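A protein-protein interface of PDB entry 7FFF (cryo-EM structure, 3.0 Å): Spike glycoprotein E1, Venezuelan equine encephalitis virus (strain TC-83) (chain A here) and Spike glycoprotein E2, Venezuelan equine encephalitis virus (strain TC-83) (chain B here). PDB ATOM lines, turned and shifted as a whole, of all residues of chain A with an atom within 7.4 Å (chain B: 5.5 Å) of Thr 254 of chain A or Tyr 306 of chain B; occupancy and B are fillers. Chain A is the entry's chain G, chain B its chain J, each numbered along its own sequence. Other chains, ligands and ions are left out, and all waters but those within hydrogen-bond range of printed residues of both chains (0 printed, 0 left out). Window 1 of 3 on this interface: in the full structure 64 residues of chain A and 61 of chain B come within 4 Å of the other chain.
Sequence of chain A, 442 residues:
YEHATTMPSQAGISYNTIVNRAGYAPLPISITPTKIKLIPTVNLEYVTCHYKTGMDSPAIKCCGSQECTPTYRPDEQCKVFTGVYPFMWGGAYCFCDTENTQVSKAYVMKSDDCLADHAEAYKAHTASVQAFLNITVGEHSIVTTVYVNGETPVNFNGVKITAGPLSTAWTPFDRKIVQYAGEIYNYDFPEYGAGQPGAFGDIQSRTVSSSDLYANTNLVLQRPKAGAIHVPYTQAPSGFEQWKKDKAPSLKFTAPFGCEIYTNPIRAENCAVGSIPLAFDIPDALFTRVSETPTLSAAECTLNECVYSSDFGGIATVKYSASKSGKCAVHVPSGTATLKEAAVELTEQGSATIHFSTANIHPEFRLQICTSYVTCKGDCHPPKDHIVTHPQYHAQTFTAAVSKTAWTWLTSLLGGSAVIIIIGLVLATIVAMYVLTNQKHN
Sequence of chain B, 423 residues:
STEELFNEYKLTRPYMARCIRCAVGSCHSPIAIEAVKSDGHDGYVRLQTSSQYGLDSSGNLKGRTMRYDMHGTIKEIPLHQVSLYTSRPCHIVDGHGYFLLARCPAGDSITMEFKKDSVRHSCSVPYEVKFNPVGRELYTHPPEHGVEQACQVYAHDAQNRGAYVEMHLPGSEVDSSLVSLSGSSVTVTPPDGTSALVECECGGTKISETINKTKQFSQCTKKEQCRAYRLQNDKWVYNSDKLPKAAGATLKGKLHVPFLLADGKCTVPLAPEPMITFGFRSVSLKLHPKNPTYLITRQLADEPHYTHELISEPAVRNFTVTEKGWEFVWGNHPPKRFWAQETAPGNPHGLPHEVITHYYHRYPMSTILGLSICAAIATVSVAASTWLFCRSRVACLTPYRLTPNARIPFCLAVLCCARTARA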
ATOM      1  N   PRO A 172     -14.690  -6.213   3.645  1.00  0.00           N
ATOM      2  CA  PRO A 172     -14.468  -6.717   5.006  1.00  0.00           C
ATOM      3  C   PRO A 172     -13.132  -7.402   5.188  1.00  0.00           C
ATOM      4  O   PRO A 172     -12.743  -7.669   6.329  1.00  0.00           O
ATOM      5  CB  PRO A 172     -15.620  -7.704   5.202  1.00  0.00           C
ATOM      6  CG  PRO A 172     -15.961  -8.139   3.845  1.00  0.00           C
ATOM      7  CD  PRO A 172     -15.759  -6.954   2.963  1.00  0.00           C
ATOM      8  N   ILE A 184     -12.750 -17.671   7.839  1.00  0.00           N
ATOM      9  CA  ILE A 184     -11.790 -16.782   7.207  1.00  0.00           C
ATOM     10  C   ILE A 184     -11.334 -15.752   8.232  1.00  0.00           C
ATOM     11  O   ILE A 184     -12.140 -15.261   9.021  1.00  0.00           O
ATOM     12  CB  ILE A 184     -12.438 -16.148   5.959  1.00  0.00           C
ATOM     13  CG1 ILE A 184     -12.626 -17.240   4.906  1.00  0.00           C
ATOM     14  CG2 ILE A 184     -11.644 -15.002   5.410  1.00  0.00           C
ATOM     15  CD1 ILE A 184     -13.505 -16.887   3.794  1.00  0.00           C
ATOM     16  N   ASN A 186      -8.793 -12.306   9.004  1.00  0.00           N
ATOM     17  CA  ASN A 186      -7.836 -11.254   8.683  1.00  0.00           C
ATOM     18  C   ASN A 186      -6.637 -11.461   9.584  1.00  0.00           C
ATOM     19  O   ASN A 186      -6.653 -11.081  10.753  1.00  0.00           O
ATOM     20  CB  ASN A 186      -8.442  -9.876   8.893  1.00  0.00           C
ATOM     21  CG  ASN A 186      -9.471  -9.537   7.863  1.00  0.00           C
ATOM     22  OD1 ASN A 186      -9.318  -9.860   6.691  1.00  0.00           O
ATOM     23  ND2 ASN A 186     -10.517  -8.852   8.281  1.00  0.00           N
ATOM     24  N   ALA A 248      -8.435 -15.506  17.553  1.00  0.00           N
ATOM     25  CA  ALA A 248      -9.485 -14.503  17.640  1.00  0.00           C
ATOM     26  C   ALA A 248     -10.545 -14.788  16.576  1.00  0.00           C
ATOM     27  O   ALA A 248     -10.187 -15.176  15.459  1.00  0.00           O
ATOM     28  CB  ALA A 248      -8.893 -13.109  17.442  1.00  0.00           C
ATOM     29  N   PRO A 249     -11.836 -14.611  16.891  1.00  0.00           N
ATOM     30  CA  PRO A 249     -12.921 -15.241  16.116  1.00  0.00           C
ATOM     31  C   PRO A 249     -12.976 -14.826  14.652  1.00  0.00           C
ATOM     32  O   PRO A 249     -12.364 -13.850  14.214  1.00  0.00           O
ATOM     33  CB  PRO A 249     -14.183 -14.787  16.851  1.00  0.00           C
ATOM     34  CG  PRO A 249     -13.744 -14.529  18.207  1.00  0.00           C
ATOM     35  CD  PRO A 249     -12.371 -13.958  18.095  1.00  0.00           C
ATOM     36  N   SER A 250     -13.767 -15.591  13.906  1.00  0.00           N
ATOM     37  CA  SER A 250     -13.772 -15.575  12.456  1.00  0.00           C
ATOM     38  C   SER A 250     -14.301 -14.260  11.920  1.00  0.00           C
ATOM     39  O   SER A 250     -14.751 -13.381  12.655  1.00  0.00           O
ATOM     40  CB  SER A 250     -14.636 -16.707  11.924  1.00  0.00           C
ATOM     41  OG  SER A 250     -14.151 -17.950  12.368  1.00  0.00           O
ATOM     42  N   LEU A 251     -14.278 -14.140  10.609  1.00  0.00           N
ATOM     43  CA  LEU A 251     -14.730 -12.889  10.045  1.00  0.00           C
ATOM     44  C   LEU A 251     -16.240 -12.862   9.887  1.00  0.00           C
ATOM     45  O   LEU A 251     -16.802 -11.799   9.638  1.00  0.00           O
ATOM     46  CB  LEU A 251     -13.998 -12.643   8.727  1.00  0.00           C
ATOM     47  CG  LEU A 251     -13.899 -11.210   8.241  1.00  0.00           C
ATOM     48  CD1 LEU A 251     -13.319 -10.407   9.365  1.00  0.00           C
ATOM     49  CD2 LEU A 251     -12.974 -11.129   7.073  1.00  0.00           C
ATOM     50  N   LYS A 252     -16.922 -13.987  10.077  1.00  0.00           N
ATOM     51  CA  LYS A 252     -18.375 -13.944  10.085  1.00  0.00           C
ATOM     52  C   LYS A 252     -18.945 -13.523  11.428  1.00  0.00           C
ATOM     53  O   LYS A 252     -20.168 -13.472  11.572  1.00  0.00           O
ATOM     54  CB  LYS A 252     -18.972 -15.292   9.698  1.00  0.00           C
ATOM     55  CG  LYS A 252     -18.695 -16.412  10.631  1.00  0.00           C
ATOM     56  CD  LYS A 252     -19.454 -17.618  10.143  1.00  0.00           C
ATOM     57  CE  LYS A 252     -19.259 -18.819  11.019  1.00  0.00           C
ATOM     58  NZ  LYS A 252     -20.061 -19.948  10.496  1.00  0.00           N
ATOM     59  N   PHE A 253     -18.095 -13.228  12.408  1.00  0.00           N
ATOM     60  CA  PHE A 253     -18.544 -12.768  13.707  1.00  0.00           C
ATOM     61  C   PHE A 253     -18.083 -11.360  14.033  1.00  0.00           C
ATOM     62  O   PHE A 253     -18.681 -10.719  14.894  1.00  0.00           O
ATOM     63  CB  PHE A 253     -18.045 -13.705  14.808  1.00  0.00           C
ATOM     64  CG  PHE A 253     -18.555 -15.109  14.692  1.00  0.00           C
ATOM     65  CD1 PHE A 253     -19.851 -15.426  15.042  1.00  0.00           C
ATOM     66  CD2 PHE A 253     -17.721 -16.120  14.272  1.00  0.00           C
ATOM     67  CE1 PHE A 253     -20.305 -16.719  14.949  1.00  0.00           C
ATOM     68  CE2 PHE A 253     -18.173 -17.410  14.178  1.00  0.00           C
ATOM     69  CZ  PHE A 253     -19.464 -17.708  14.517  1.00  0.00           C
ATOM     70  N   THR A 254     -17.042 -10.867  13.368  1.00  0.00           N
ATOM     71  CA  THR A 254     -16.460  -9.573  13.671  1.00  0.00           C
ATOM     72  C   THR A 254     -16.594  -8.567  12.539  1.00  0.00           C
ATOM     73  O   THR A 254     -16.117  -7.440  12.683  1.00  0.00           O
ATOM     74  CB  THR A 254     -14.973  -9.726  14.004  1.00  0.00           C
ATOM     75  OG1 THR A 254     -14.270 -10.124  12.830  1.00  0.00           O
ATOM     76  CG2 THR A 254     -14.772 -10.770  15.060  1.00  0.00           C
ATOM     77  N   ALA A 255     -17.204  -8.932  11.420  1.00  0.00           N
ATOM     78  CA  ALA A 255     -17.200  -7.987  10.310  1.00  0.00           C
ATOM     79  C   ALA A 255     -18.307  -6.958  10.494  1.00  0.00           C
ATOM     80  O   ALA A 255     -19.408  -7.304  10.918  1.00  0.00           O
ATOM     81  CB  ALA A 255     -17.390  -8.694   8.980  1.00  0.00           C
ATOM     82  N   PRO A 256     -18.041  -5.695  10.190  1.00  0.00           N
ATOM     83  CA  PRO A 256     -19.104  -4.687  10.258  1.00  0.00           C
ATOM     84  C   PRO A 256     -20.093  -4.780   9.114  1.00  0.00           C
ATOM     85  O   PRO A 256     -19.953  -5.628   8.230  1.00  0.00           O
ATOM     86  CB  PRO A 256     -18.329  -3.369  10.226  1.00  0.00           C
ATOM     87  CG  PRO A 256     -17.066  -3.692   9.587  1.00  0.00           C
ATOM     88  CD  PRO A 256     -16.726  -5.089   9.945  1.00  0.00           C
ATOM     89  N   PHE A 257     -21.119  -3.927   9.158  1.00  0.00           N
ATOM     90  CA  PHE A 257     -22.175  -3.796   8.150  1.00  0.00           C
ATOM     91  C   PHE A 257     -22.967  -5.080   7.931  1.00  0.00           C
ATOM     92  O   PHE A 257     -23.589  -5.247   6.882  1.00  0.00           O
ATOM     93  CB  PHE A 257     -21.615  -3.289   6.814  1.00  0.00           C
ATOM     94  CG  PHE A 257     -21.105  -1.882   6.871  1.00  0.00           C
ATOM     95  CD1 PHE A 257     -21.981  -0.820   6.823  1.00  0.00           C
ATOM     96  CD2 PHE A 257     -19.752  -1.623   6.986  1.00  0.00           C
ATOM     97  CE1 PHE A 257     -21.517   0.473   6.881  1.00  0.00           C
ATOM     98  CE2 PHE A 257     -19.285  -0.329   7.044  1.00  0.00           C
ATOM     99  CZ  PHE A 257     -20.163   0.714   6.986  1.00  0.00           C
ATOM    100  N   CYS A 259     -22.136  -8.315   7.521  1.00  0.00           N
ATOM    101  CA  CYS A 259     -21.711  -9.151   6.412  1.00  0.00           C
ATOM    102  C   CYS A 259     -21.688 -10.617   6.822  1.00  0.00           C
ATOM    103  O   CYS A 259     -21.533 -10.959   7.992  1.00  0.00           O
ATOM    104  CB  CYS A 259     -20.333  -8.724   5.925  1.00  0.00           C
ATOM    105  SG  CYS A 259     -20.282  -7.053   5.318  1.00  0.00           S
ATOM    106  N   ILE A 261     -19.758 -13.998   5.893  1.00  0.00           N
ATOM    107  CA  ILE A 261     -18.602 -14.530   5.180  1.00  0.00           C
ATOM    108  C   ILE A 261     -18.845 -15.995   4.840  1.00  0.00           C
ATOM    109  O   ILE A 261     -19.033 -16.824   5.734  1.00  0.00           O
ATOM    110  CB  ILE A 261     -17.321 -14.368   6.003  1.00  0.00           C
ATOM    111  CG1 ILE A 261     -17.136 -12.920   6.439  1.00  0.00           C
ATOM    112  CG2 ILE A 261     -16.153 -14.768   5.181  1.00  0.00           C
ATOM    113  CD1 ILE A 261     -17.037 -11.950   5.315  1.00  0.00           C
ATOM    114  N   THR B 297     -21.665 -11.445  20.242  1.00  0.00           N
ATOM    115  CA  THR B 297     -22.510 -10.400  19.679  1.00  0.00           C
ATOM    116  C   THR B 297     -21.690  -9.480  18.785  1.00  0.00           C
ATOM    117  O   THR B 297     -20.462  -9.442  18.871  1.00  0.00           O
ATOM    118  CB  THR B 297     -23.173  -9.552  20.763  1.00  0.00           C
ATOM    119  OG1 THR B 297     -22.181  -8.758  21.407  1.00  0.00           O
ATOM    120  CG2 THR B 297     -23.804 -10.418  21.804  1.00  0.00           C
ATOM    121  N   ARG B 298     -22.389  -8.728  17.929  1.00  0.00           N
ATOM    122  CA  ARG B 298     -21.807  -7.664  17.109  1.00  0.00           C
ATOM    123  C   ARG B 298     -22.929  -6.794  16.574  1.00  0.00           C
ATOM    124  O   ARG B 298     -24.034  -7.278  16.331  1.00  0.00           O
ATOM    125  CB  ARG B 298     -20.943  -8.202  15.954  1.00  0.00           C
ATOM    126  CG  ARG B 298     -21.598  -9.135  14.924  1.00  0.00           C
ATOM    127  CD  ARG B 298     -21.971  -8.437  13.629  1.00  0.00           C
ATOM    128  NE  ARG B 298     -22.481  -9.374  12.634  1.00  0.00           N
ATOM    129  CZ  ARG B 298     -21.778  -9.843  11.610  1.00  0.00           C
ATOM    130  NH1 ARG B 298     -20.542  -9.433  11.405  1.00  0.00           N
ATOM    131  NH2 ARG B 298     -22.331 -10.692  10.760  1.00  0.00           N
ATOM    132  N   PRO B 304     -18.704  -2.390  14.634  1.00  0.00           N
ATOM    133  CA  PRO B 304     -19.589  -3.375  15.257  1.00  0.00           C
ATOM    134  C   PRO B 304     -19.448  -3.488  16.766  1.00  0.00           C
ATOM    135  O   PRO B 304     -20.444  -3.790  17.428  1.00  0.00           O
ATOM    136  CB  PRO B 304     -19.185  -4.678  14.566  1.00  0.00           C
ATOM    137  CG  PRO B 304     -17.784  -4.471  14.193  1.00  0.00           C
ATOM    138  CD  PRO B 304     -17.641  -3.028  13.847  1.00  0.00           C
ATOM    139  N   HIS B 305     -18.252  -3.242  17.309  1.00  0.00           N
ATOM    140  CA  HIS B 305     -17.903  -3.487  18.713  1.00  0.00           C
ATOM    141  C   HIS B 305     -18.263  -4.916  19.123  1.00  0.00           C
ATOM    142  O   HIS B 305     -19.181  -5.147  19.906  1.00  0.00           O
ATOM    143  CB  HIS B 305     -18.571  -2.487  19.666  1.00  0.00           C
ATOM    144  CG  HIS B 305     -18.203  -1.060  19.417  1.00  0.00           C
ATOM    145  ND1 HIS B 305     -16.944  -0.561  19.664  1.00  0.00           N
ATOM    146  CD2 HIS B 305     -18.945  -0.012  18.988  1.00  0.00           C
ATOM    147  CE1 HIS B 305     -16.918   0.726  19.370  1.00  0.00           C
ATOM    148  NE2 HIS B 305     -18.119   1.084  18.959  1.00  0.00           N
ATOM    149  N   TYR B 306     -17.558  -5.872  18.524  1.00  0.00           N
ATOM    150  CA  TYR B 306     -17.916  -7.265  18.732  1.00  0.00           C
ATOM    151  C   TYR B 306     -17.533  -7.694  20.136  1.00  0.00           C
ATOM    152  O   TYR B 306     -16.600  -7.165  20.742  1.00  0.00           O
ATOM    153  CB  TYR B 306     -17.242  -8.172  17.699  1.00  0.00           C
ATOM    154  CG  TYR B 306     -15.758  -8.362  17.883  1.00  0.00           C
ATOM    155  CD1 TYR B 306     -14.861  -7.437  17.383  1.00  0.00           C
ATOM    156  CD2 TYR B 306     -15.252  -9.498  18.505  1.00  0.00           C
ATOM    157  CE1 TYR B 306     -13.513  -7.608  17.540  1.00  0.00           C
ATOM    158  CE2 TYR B 306     -13.913  -9.675  18.669  1.00  0.00           C
ATOM    159  CZ  TYR B 306     -13.043  -8.732  18.182  1.00  0.00           C
ATOM    160  OH  TYR B 306     -11.689  -8.903  18.333  1.00  0.00           O
ATOM    161  N   THR B 307     -18.267  -8.667  20.649  1.00  0.00           N
ATOM    162  CA  THR B 307     -18.098  -9.130  22.013  1.00  0.00           C
ATOM    163  C   THR B 307     -17.990 -10.639  21.995  1.00  0.00           C
ATOM    164  O   THR B 307     -18.876 -11.319  21.481  1.00  0.00           O
ATOM    165  CB  THR B 307     -19.272  -8.699  22.880  1.00  0.00           C
ATOM    166  OG1 THR B 307     -19.424  -7.280  22.804  1.00  0.00           O
ATOM    167  CG2 THR B 307     -19.030  -9.081  24.310  1.00  0.00           C
ATOM    168  N   HIS B 308     -16.912 -11.161  22.560  1.00  0.00           N
ATOM    169  CA  HIS B 308     -16.660 -12.592  22.608  1.00  0.00           C
ATOM    170  C   HIS B 308     -16.513 -12.977  24.068  1.00  0.00           C
ATOM    171  O   HIS B 308     -15.697 -12.386  24.781  1.00  0.00           O
ATOM    172  CB  HIS B 308     -15.404 -12.928  21.809  1.00  0.00           C
ATOM    173  CG  HIS B 308     -15.061 -14.379  21.790  1.00  0.00           C
ATOM    174  ND1 HIS B 308     -15.796 -15.306  21.092  1.00  0.00           N
ATOM    175  CD2 HIS B 308     -14.036 -15.056  22.356  1.00  0.00           C
ATOM    176  CE1 HIS B 308     -15.249 -16.498  21.237  1.00  0.00           C
ATOM    177  NE2 HIS B 308     -14.181 -16.374  22.004  1.00  0.00           N
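Printed residues of chain B within 4 Å of Phe 253 of chain A: Arg 298. Printed residues of chain B within 4 Å of Thr 254 of chain A: Pro 304 and Tyr 306. Of the printed residues of chain B, Pro 256 of chain A touches Pro 304 (3.7 Å). Of the printed residues of chain A, Pro 304 of chain B touches Thr 254 and Pro 256. Of chain A, only Thr 254 (3.7 Å) comes within 4 Å of Tyr 306 of chain B. The nearest residue of chain B that does not touch Thr 254 of chain A is Arg 298 of chain B (4.2 Å). The nearest residue of chain A that does not touch Tyr 306 of chain B is Phe 253 of chain A (4.1 Å). The nearest printed residue of chain A that does not touch His 308 of chain B is Ala 248 of chain A (6.6 Å).
The side-chain hydroxyl (OG1) of Thr 254 of chain A is in hydrogen-bond range of the backbone carbonyl oxygen (O) of Ser 250 of chain A (3.3 Å).
Among the printed residues, pairs that only touch across the chains: Phe 253 of chain A with Arg 298 of chain B (3.3 Å), Lys 252 of chain A with Arg 298 of chain B (3.6 Å), Pro 249 of chain A with His 308 of chain B (3.6 Å), Pro 256 of chain A with Pro 304 of chain B (3.7 Å), Thr 254 of chain A with Tyr 306 of chain B (3.7 Å) and Thr 254 of chain A with Pro 304 of chain B (3.7 Å).
Hydrophobic or aromatic side chains of chain B within 4 Å of the printed part of chain A: Pro 304, Tyr 306 and His 308. Of the 15 printed residues of chain A, 7 touch a printed residue of chain B. Hydrophobic or aromatic side chains of chain A that line the printed part of chain B: Pro 249 and Pro 256. Among the printed residues, no Asp or Glu carboxylate lies within 4 Å of a Lys or Arg side-chain nitrogen of the other chain.
O of Ala 255 of chain A is in hydrogen-bond range of NH1 of Arg 298 of chain B, 2.5 Å away. The guanidinium group (NH2) of Arg 298 of chain B is in hydrogen-bond range of the backbone carbonyl oxygen (O) of Cys 259 of chain A (2.9 Å).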
